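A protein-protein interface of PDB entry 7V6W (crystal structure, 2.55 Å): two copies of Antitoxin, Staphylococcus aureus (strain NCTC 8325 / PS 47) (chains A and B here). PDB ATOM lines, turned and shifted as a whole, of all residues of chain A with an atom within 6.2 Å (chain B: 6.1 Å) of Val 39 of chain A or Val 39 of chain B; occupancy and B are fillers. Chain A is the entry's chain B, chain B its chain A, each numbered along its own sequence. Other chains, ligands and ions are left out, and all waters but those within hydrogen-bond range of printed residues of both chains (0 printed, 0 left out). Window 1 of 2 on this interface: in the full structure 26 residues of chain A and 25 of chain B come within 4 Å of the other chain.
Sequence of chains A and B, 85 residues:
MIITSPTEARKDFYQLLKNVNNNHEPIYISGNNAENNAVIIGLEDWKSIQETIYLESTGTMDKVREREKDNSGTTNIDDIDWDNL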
ATOM      1  N   LEU A  17       6.885  -2.446 -18.317  1.00  0.00           N
ATOM      2  CA  LEU A  17       7.943  -3.441 -18.463  1.00  0.00           C
ATOM      3  C   LEU A  17       9.076  -2.930 -19.341  1.00  0.00           C
ATOM      4  O   LEU A  17      10.230  -3.342 -19.167  1.00  0.00           O
ATOM      5  CB  LEU A  17       7.370  -4.737 -19.038  1.00  0.00           C
ATOM      6  CG  LEU A  17       6.355  -5.479 -18.167  1.00  0.00           C
ATOM      7  CD1 LEU A  17       5.838  -6.719 -18.883  1.00  0.00           C
ATOM      8  CD2 LEU A  17       6.969  -5.845 -16.824  1.00  0.00           C
ATOM      9  N   PRO A  26      13.242   1.198 -10.783  1.00  0.00           N
ATOM     10  CA  PRO A  26      12.118   0.344 -10.384  1.00  0.00           C
ATOM     11  C   PRO A  26      10.802   1.106 -10.369  1.00  0.00           C
ATOM     12  O   PRO A  26      10.750   2.307 -10.093  1.00  0.00           O
ATOM     13  CB  PRO A  26      12.504  -0.118  -8.973  1.00  0.00           C
ATOM     14  CG  PRO A  26      13.976   0.155  -8.854  1.00  0.00           C
ATOM     15  CD  PRO A  26      14.225   1.359  -9.700  1.00  0.00           C
ATOM     16  N   ILE A  27       9.727   0.385 -10.678  1.00  0.00           N
ATOM     17  CA  ILE A  27       8.368   0.909 -10.602  1.00  0.00           C
ATOM     18  C   ILE A  27       7.732   0.365  -9.331  1.00  0.00           C
ATOM     19  O   ILE A  27       7.688  -0.853  -9.123  1.00  0.00           O
ATOM     20  CB  ILE A  27       7.539   0.525 -11.836  1.00  0.00           C
ATOM     21  CG1 ILE A  27       8.251   0.943 -13.123  1.00  0.00           C
ATOM     22  CG2 ILE A  27       6.155   1.155 -11.765  1.00  0.00           C
ATOM     23  CD1 ILE A  27       8.524   2.420 -13.227  1.00  0.00           C
ATOM     24  N   TYR A  28       7.242   1.261  -8.482  1.00  0.00           N
ATOM     25  CA  TYR A  28       6.611   0.885  -7.225  1.00  0.00           C
ATOM     26  C   TYR A  28       5.101   0.820  -7.412  1.00  0.00           C
ATOM     27  O   TYR A  28       4.494   1.756  -7.943  1.00  0.00           O
ATOM     28  CB  TYR A  28       6.969   1.878  -6.118  1.00  0.00           C
ATOM     29  CG  TYR A  28       8.404   1.768  -5.651  1.00  0.00           C
ATOM     30  CD1 TYR A  28       9.414   2.504  -6.257  1.00  0.00           C
ATOM     31  CD2 TYR A  28       8.746   0.922  -4.604  1.00  0.00           C
ATOM     32  CE1 TYR A  28      10.727   2.400  -5.832  1.00  0.00           C
ATOM     33  CE2 TYR A  28      10.054   0.812  -4.173  1.00  0.00           C
ATOM     34  CZ  TYR A  28      11.040   1.553  -4.788  1.00  0.00           C
ATOM     35  OH  TYR A  28      12.342   1.441  -4.355  1.00  0.00           O
ATOM     36  N   ILE A  29       4.503  -0.284  -6.978  1.00  0.00           N
ATOM     37  CA  ILE A  29       3.066  -0.501  -7.080  1.00  0.00           C
ATOM     38  C   ILE A  29       2.483  -0.379  -5.679  1.00  0.00           C
ATOM     39  O   ILE A  29       2.710  -1.243  -4.823  1.00  0.00           O
ATOM     40  CB  ILE A  29       2.736  -1.862  -7.707  1.00  0.00           C
ATOM     41  CG1 ILE A  29       3.253  -1.923  -9.145  1.00  0.00           C
ATOM     42  CG2 ILE A  29       1.243  -2.130  -7.655  1.00  0.00           C
ATOM     43  CD1 ILE A  29       2.973  -3.234  -9.837  1.00  0.00           C
ATOM     44  N   ASN A  37       1.311  -4.543  -2.045  1.00  0.00           N
ATOM     45  CA  ASN A  37       2.240  -3.668  -2.743  1.00  0.00           C
ATOM     46  C   ASN A  37       3.440  -4.456  -3.255  1.00  0.00           C
ATOM     47  O   ASN A  37       3.885  -5.428  -2.638  1.00  0.00           O
ATOM     48  CB  ASN A  37       2.705  -2.538  -1.824  1.00  0.00           C
ATOM     49  CG  ASN A  37       1.637  -1.482  -1.613  1.00  0.00           C
ATOM     50  OD1 ASN A  37       0.504  -1.631  -2.070  1.00  0.00           O
ATOM     51  ND2 ASN A  37       1.992  -0.409  -0.916  1.00  0.00           N
ATOM     52  N   ALA A  38       3.964  -4.025  -4.400  1.00  0.00           N
ATOM     53  CA  ALA A  38       5.051  -4.729  -5.062  1.00  0.00           C
ATOM     54  C   ALA A  38       5.913  -3.720  -5.810  1.00  0.00           C
ATOM     55  O   ALA A  38       5.614  -2.524  -5.850  1.00  0.00           O
ATOM     56  CB  ALA A  38       4.512  -5.812  -6.003  1.00  0.00           C
ATOM     57  N   VAL A  39       6.994  -4.217  -6.409  1.00  0.00           N
ATOM     58  CA  VAL A  39       7.914  -3.398  -7.188  1.00  0.00           C
ATOM     59  C   VAL A  39       8.329  -4.179  -8.429  1.00  0.00           C
ATOM     60  O   VAL A  39       8.504  -5.402  -8.379  1.00  0.00           O
ATOM     61  CB  VAL A  39       9.142  -2.976  -6.348  1.00  0.00           C
ATOM     62  CG1 VAL A  39       9.909  -4.195  -5.867  1.00  0.00           C
ATOM     63  CG2 VAL A  39      10.048  -2.048  -7.142  1.00  0.00           C
ATOM     64  N   ILE A  40       8.471  -3.473  -9.550  1.00  0.00           N
ATOM     65  CA  ILE A  40       8.872  -4.062 -10.823  1.00  0.00           C
ATOM     66  C   ILE A  40      10.294  -3.614 -11.129  1.00  0.00           C
ATOM     67  O   ILE A  40      10.584  -2.411 -11.137  1.00  0.00           O
ATOM     68  CB  ILE A  40       7.922  -3.655 -11.963  1.00  0.00           C
ATOM     69  CG1 ILE A  40       6.465  -3.687 -11.493  1.00  0.00           C
ATOM     70  CG2 ILE A  40       8.121  -4.561 -13.170  1.00  0.00           C
ATOM     71  CD1 ILE A  40       5.991  -5.047 -11.060  1.00  0.00           C
ATOM     72  N   ILE A  41      11.178  -4.577 -11.385  1.00  0.00           N
ATOM     73  CA  ILE A  41      12.582  -4.306 -11.669  1.00  0.00           C
ATOM     74  C   ILE A  41      12.972  -5.038 -12.945  1.00  0.00           C
ATOM     75  O   ILE A  41      12.558  -6.181 -13.167  1.00  0.00           O
ATOM     76  CB  ILE A  41      13.494  -4.735 -10.498  1.00  0.00           C
ATOM     77  CG1 ILE A  41      13.074  -4.029  -9.210  1.00  0.00           C
ATOM     78  CG2 ILE A  41      14.953  -4.438 -10.806  1.00  0.00           C
ATOM     79  CD1 ILE A  41      12.776  -4.978  -8.078  1.00  0.00           C
ATOM     80  N   GLY A  42      13.763  -4.375 -13.787  1.00  0.00           N
ATOM     81  CA  GLY A  42      14.267  -5.026 -14.981  1.00  0.00           C
ATOM     82  C   GLY A  42      15.121  -6.233 -14.645  1.00  0.00           C
ATOM     83  O   GLY A  42      15.788  -6.286 -13.609  1.00  0.00           O
ATOM     84  N   LEU A  43      15.100  -7.217 -15.547  1.00  0.00           N
ATOM     85  CA  LEU A  43      15.765  -8.488 -15.277  1.00  0.00           C
ATOM     86  C   LEU A  43      17.275  -8.314 -15.149  1.00  0.00           C
ATOM     87  O   LEU A  43      17.894  -8.863 -14.230  1.00  0.00           O
ATOM     88  CB  LEU A  43      15.430  -9.496 -16.377  1.00  0.00           C
ATOM     89  CG  LEU A  43      16.078 -10.867 -16.190  1.00  0.00           C
ATOM     90  CD1 LEU A  43      15.657 -11.459 -14.856  1.00  0.00           C
ATOM     91  CD2 LEU A  43      15.723 -11.799 -17.338  1.00  0.00           C
ATOM     92  N   TRP A  46      18.018  -6.789 -11.919  1.00  0.00           N
ATOM     93  CA  TRP A  46      17.731  -7.686 -10.805  1.00  0.00           C
ATOM     94  C   TRP A  46      18.835  -8.718 -10.602  1.00  0.00           C
ATOM     95  O   TRP A  46      19.066  -9.156  -9.470  1.00  0.00           O
ATOM     96  CB  TRP A  46      16.388  -8.383 -11.029  1.00  0.00           C
ATOM     97  CG  TRP A  46      16.172  -9.586 -10.159  1.00  0.00           C
ATOM     98  CD1 TRP A  46      16.291 -10.895 -10.526  1.00  0.00           C
ATOM     99  CD2 TRP A  46      15.804  -9.590  -8.774  1.00  0.00           C
ATOM    100  NE1 TRP A  46      16.017 -11.714  -9.458  1.00  0.00           N
ATOM    101  CE2 TRP A  46      15.716 -10.937  -8.370  1.00  0.00           C
ATOM    102  CE3 TRP A  46      15.538  -8.587  -7.838  1.00  0.00           C
ATOM    103  CZ2 TRP A  46      15.373 -11.306  -7.071  1.00  0.00           C
ATOM    104  CZ3 TRP A  46      15.199  -8.955  -6.549  1.00  0.00           C
ATOM    105  CH2 TRP A  46      15.119 -10.303  -6.177  1.00  0.00           C
ATOM    106  N   PRO B  26      10.096 -14.131  -5.990  1.00  0.00           N
ATOM    107  CA  PRO B  26      10.015 -13.271  -7.173  1.00  0.00           C
ATOM    108  C   PRO B  26       9.286 -13.970  -8.310  1.00  0.00           C
ATOM    109  O   PRO B  26       9.272 -15.198  -8.409  1.00  0.00           O
ATOM    110  CB  PRO B  26      11.484 -13.014  -7.525  1.00  0.00           C
ATOM    111  CG  PRO B  26      12.219 -13.222  -6.237  1.00  0.00           C
ATOM    112  CD  PRO B  26      11.484 -14.325  -5.538  1.00  0.00           C
ATOM    113  N   ILE B  27       8.666 -13.169  -9.170  1.00  0.00           N
ATOM    114  CA  ILE B  27       7.955 -13.667 -10.340  1.00  0.00           C
ATOM    115  C   ILE B  27       8.584 -13.029 -11.569  1.00  0.00           C
ATOM    116  O   ILE B  27       8.591 -11.800 -11.704  1.00  0.00           O
ATOM    117  CB  ILE B  27       6.450 -13.376 -10.268  1.00  0.00           C
ATOM    118  CG1 ILE B  27       5.827 -14.149  -9.101  1.00  0.00           C
ATOM    119  CG2 ILE B  27       5.776 -13.736 -11.586  1.00  0.00           C
ATOM    120  CD1 ILE B  27       4.336 -13.967  -8.953  1.00  0.00           C
ATOM    121  N   TYR B  28       9.116 -13.864 -12.456  1.00  0.00           N
ATOM    122  CA  TYR B  28       9.840 -13.397 -13.629  1.00  0.00           C
ATOM    123  C   TYR B  28       8.876 -13.261 -14.799  1.00  0.00           C
ATOM    124  O   TYR B  28       8.173 -14.216 -15.148  1.00  0.00           O
ATOM    125  CB  TYR B  28      10.983 -14.353 -13.969  1.00  0.00           C
ATOM    126  CG  TYR B  28      12.036 -14.442 -12.886  1.00  0.00           C
ATOM    127  CD1 TYR B  28      11.837 -15.228 -11.758  1.00  0.00           C
ATOM    128  CD2 TYR B  28      13.228 -13.739 -12.991  1.00  0.00           C
ATOM    129  CE1 TYR B  28      12.794 -15.309 -10.765  1.00  0.00           C
ATOM    130  CE2 TYR B  28      14.192 -13.814 -12.003  1.00  0.00           C
ATOM    131  CZ  TYR B  28      13.970 -14.601 -10.893  1.00  0.00           C
ATOM    132  OH  TYR B  28      14.926 -14.681  -9.906  1.00  0.00           O
ATOM    133  N   ILE B  29       8.839 -12.073 -15.393  1.00  0.00           N
ATOM    134  CA  ILE B  29       8.012 -11.793 -16.559  1.00  0.00           C
ATOM    135  C   ILE B  29       8.892 -11.930 -17.793  1.00  0.00           C
ATOM    136  O   ILE B  29       9.904 -11.233 -17.922  1.00  0.00           O
ATOM    137  CB  ILE B  29       7.381 -10.395 -16.479  1.00  0.00           C
ATOM    138  CG1 ILE B  29       6.710 -10.185 -15.120  1.00  0.00           C
ATOM    139  CG2 ILE B  29       6.380 -10.202 -17.600  1.00  0.00           C
ATOM    140  CD1 ILE B  29       5.606 -11.174 -14.827  1.00  0.00           C
ATOM    141  N   ASN B  37      11.357  -8.141 -20.243  1.00  0.00           N
ATOM    142  CA  ASN B  37      11.928  -8.982 -19.200  1.00  0.00           C
ATOM    143  C   ASN B  37      12.097  -8.203 -17.905  1.00  0.00           C
ATOM    144  O   ASN B  37      12.865  -7.239 -17.844  1.00  0.00           O
ATOM    145  CB  ASN B  37      13.266  -9.549 -19.668  1.00  0.00           C
ATOM    146  CG  ASN B  37      13.096 -10.658 -20.684  1.00  0.00           C
ATOM    147  OD1 ASN B  37      12.049 -11.303 -20.739  1.00  0.00           O
ATOM    148  ND2 ASN B  37      14.126 -10.892 -21.490  1.00  0.00           N
ATOM    149  N   ALA B  38      11.377  -8.628 -16.871  1.00  0.00           N
ATOM    150  CA  ALA B  38      11.377  -7.933 -15.595  1.00  0.00           C
ATOM    151  C   ALA B  38      11.047  -8.923 -14.488  1.00  0.00           C
ATOM    152  O   ALA B  38      10.642 -10.060 -14.738  1.00  0.00           O
ATOM    153  CB  ALA B  38      10.383  -6.768 -15.597  1.00  0.00           C
ATOM    154  N   VAL B  39      11.232  -8.473 -13.249  1.00  0.00           N
ATOM    155  CA  VAL B  39      10.946  -9.274 -12.068  1.00  0.00           C
ATOM    156  C   VAL B  39      10.007  -8.486 -11.167  1.00  0.00           C
ATOM    157  O   VAL B  39      10.079  -7.255 -11.089  1.00  0.00           O
ATOM    158  CB  VAL B  39      12.233  -9.664 -11.305  1.00  0.00           C
ATOM    159  CG1 VAL B  39      11.963 -10.826 -10.370  1.00  0.00           C
ATOM    160  CG2 VAL B  39      13.349 -10.009 -12.277  1.00  0.00           C
ATOM    161  N   ILE B  40       9.117  -9.203 -10.486  1.00  0.00           N
ATOM    162  CA  ILE B  40       8.124  -8.605  -9.601  1.00  0.00           C
ATOM    163  C   ILE B  40       8.396  -9.100  -8.187  1.00  0.00           C
ATOM    164  O   ILE B  40       8.361 -10.308  -7.928  1.00  0.00           O
ATOM    165  CB  ILE B  40       6.693  -8.946 -10.043  1.00  0.00           C
ATOM    166  CG1 ILE B  40       6.499  -8.549 -11.510  1.00  0.00           C
ATOM    167  CG2 ILE B  40       5.673  -8.254  -9.148  1.00  0.00           C
ATOM    168  CD1 ILE B  40       5.086  -8.679 -12.010  1.00  0.00           C
ATOM    169  N   ILE B  41       8.676  -8.165  -7.280  1.00  0.00           N
ATOM    170  CA  ILE B  41       9.019  -8.471  -5.897  1.00  0.00           C
ATOM    171  C   ILE B  41       7.986  -7.829  -4.985  1.00  0.00           C
ATOM    172  O   ILE B  41       7.469  -6.745  -5.274  1.00  0.00           O
ATOM    173  CB  ILE B  41      10.432  -7.968  -5.527  1.00  0.00           C
ATOM    174  CG1 ILE B  41      11.390  -8.118  -6.706  1.00  0.00           C
ATOM    175  CG2 ILE B  41      10.962  -8.709  -4.309  1.00  0.00           C
ATOM    176  CD1 ILE B  41      11.720  -9.542  -7.035  1.00  0.00           C
ATOM    177  N   GLY B  42       7.693  -8.498  -3.873  1.00  0.00           N
ATOM    178  CA  GLY B  42       6.892  -7.873  -2.838  1.00  0.00           C
ATOM    179  C   GLY B  42       7.622  -6.701  -2.211  1.00  0.00           C
ATOM    180  O   GLY B  42       8.848  -6.689  -2.094  1.00  0.00           O
ATOM    181  N   LEU B  43       6.850  -5.690  -1.806  1.00  0.00           N
ATOM    182  CA  LEU B  43       7.459  -4.470  -1.283  1.00  0.00           C
ATOM    183  C   LEU B  43       8.213  -4.733   0.016  1.00  0.00           C
ATOM    184  O   LEU B  43       9.320  -4.216   0.209  1.00  0.00           O
ATOM    185  CB  LEU B  43       6.397  -3.389  -1.077  1.00  0.00           C
ATOM    186  CG  LEU B  43       6.933  -2.043  -0.578  1.00  0.00           C
ATOM    187  CD1 LEU B  43       7.952  -1.467  -1.554  1.00  0.00           C
ATOM    188  CD2 LEU B  43       5.801  -1.058  -0.341  1.00  0.00           C
ATOM    189  N   TRP B  46      11.300  -6.407  -0.890  1.00  0.00           N
ATOM    190  CA  TRP B  46      12.174  -5.458  -1.571  1.00  0.00           C
ATOM    191  C   TRP B  46      12.842  -4.509  -0.584  1.00  0.00           C
ATOM    192  O   TRP B  46      14.027  -4.188  -0.729  1.00  0.00           O
ATOM    193  CB  TRP B  46      11.382  -4.672  -2.616  1.00  0.00           C
ATOM    194  CG  TRP B  46      12.116  -3.489  -3.166  1.00  0.00           C
ATOM    195  CD1 TRP B  46      11.859  -2.173  -2.907  1.00  0.00           C
ATOM    196  CD2 TRP B  46      13.229  -3.511  -4.067  1.00  0.00           C
ATOM    197  NE1 TRP B  46      12.741  -1.375  -3.594  1.00  0.00           N
ATOM    198  CE2 TRP B  46      13.593  -2.172  -4.312  1.00  0.00           C
ATOM    199  CE3 TRP B  46      13.953  -4.532  -4.690  1.00  0.00           C
ATOM    200  CZ2 TRP B  46      14.648  -1.827  -5.154  1.00  0.00           C
ATOM    201  CZ3 TRP B  46      15.002  -4.188  -5.524  1.00  0.00           C
ATOM    202  CH2 TRP B  46      15.339  -2.848  -5.749  1.00  0.00           C
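The side-chain hydroxyl (OH) of Tyr 28 of chain A lies within hydrogen-bond range of the indole nitrogen (NE1) of Trp 46 of chain B.
The backbone NH (N) of Val 39 of chain B sits at hydrogen-bond distance from the backbone carbonyl oxygen (O) of Ile 41 of chain A (2.6 Å).
The backbone carbonyl oxygen (O) of Asn 37 of chain A sits at hydrogen-bond distance from the backbone NH (N) of Leu 43 of chain B (3.1 Å).
The backbone NH (N) of Leu 43 of chain A sits at hydrogen-bond distance from the backbone carbonyl oxygen (O) of Asn 37 of chain B.
N of Val 39 of chain A sits at hydrogen-bond distance from O of Ile 41 of chain B, at 2.8 Å.
The side-chain hydroxyl (OH) of Tyr 28 of chain B lies within hydrogen-bond range of the indole nitrogen (NE1) of Trp 46 of chain A, at 3.2 Å.
O of Ala 38 of chain A is in hydrogen-bond range of N of Ile 29 of chain A, 2.7 Å away.
O of Ile 27 of chain B lies within hydrogen-bond range of N of Ile 40 of chain B (2.9 Å).
The backbone NH of Ile 29 of chain B sits at hydrogen-bond distance from the backbone carbonyl oxygen of Ala 38 of chain B (2.8 Å).
O of Ile 27 of chain A sits at hydrogen-bond distance from N of Ile 40 of chain A.
Among the printed residues, merely in contact across the chains: Ala 38 of chain A with Ile 41 of chain B (3.2 Å), Ile 41 of chain A with Ala 38 of chain B (3.2 Å), Ile 40 of chain A with Val 39 of chain B (3.4 Å), Val 39 of chain A with Ile 40 of chain B (3.4 Å), Ile 41 of chain A with Trp 46 of chain B (3.5 Å), Trp 46 of chain A with Val 39 of chain B (3.5 Å), Val 39 of chain A with Trp 46 of chain B (3.6 Å), Trp 46 of chain A with Ile 41 of chain B (3.6 Å), Ile 40 of chain A with Ile 40 of chain B (3.6 Å), Val 39 of chain A with Val 39 of chain B (3.6 Å), Ile 41 of chain A with Ile 41 of chain B (3.7 Å), Leu 17 of chain A with Ala 38 of chain B (3.7 Å), Leu 17 of chain A with Ile 29 of chain B (3.8 Å), Leu 43 of chain A with Val 39 of chain B (3.8 Å), Trp 46 of chain A with Pro 26 of chain B (3.8 Å), Leu 43 of chain A with Ala 38 of chain B (3.8 Å), Leu 43 of chain A with Tyr 28 of chain B (3.8 Å), Ala 38 of chain A with Leu 43 of chain B (3.8 Å), Gly 42 of chain A with Asn 37 of chain B (3.9 Å), Asn 37 of chain A with Gly 42 of chain B (3.9 Å), Tyr 28 of chain A with Leu 43 of chain B (3.95 Å) and Ile 40 of chain A with Ala 38 of chain B (3.98 Å).
Ala 38 of chain A touches Ile 41 of chain B, and with the chains exchanged Ile 41 of chain A touches Ala 38 of chain B.
Val 39 of chain A touches Ile 40 of chain B, and with the chains exchanged Ile 40 of chain A touches Val 39 of chain B.
Val 39 of chain A touches Trp 46 of chain B, and with the chains exchanged Trp 46 of chain A touches Val 39 of chain B.
Ile 41 of chain A touches Trp 46 of chain B, and with the chains exchanged Trp 46 of chain A touches Ile 41 of chain B.
Hydrophobic or aromatic side chains of chain B that line the printed part of chain A: Pro 26, Tyr 28, Ile 29, Ala 38, Val 39, Ile 40, Ile 41, Leu 43 and Trp 46.
Of chain B, only Val 39, Ile 40, Ile 41 and Trp 46 come within 4 Å of Val 39 of chain A.
Printed residues of chain B within 4 Å of Leu 43 of chain A: Tyr 28 (3.8 Å), Asn 37 (3.2 Å), Ala 38 (3.8 Å) and Val 39 (3.8 Å).
Val 39 of chain B touches five residues of chain A.
Of the printed residues of chain A, Gly 42 of chain B touches Asn 37 (3.9 Å).
The nearest residue of chain B that does not touch Val 39 of chain A is Gly 42 of chain B (4.6 Å).
The nearest residue of chain A that does not touch Val 39 of chain B is Gly 42 of chain A (4.6 Å).
The nearest printed residue of chain A that does not touch Pro 26 of chain B is Val 39 of chain A (8.1 Å).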
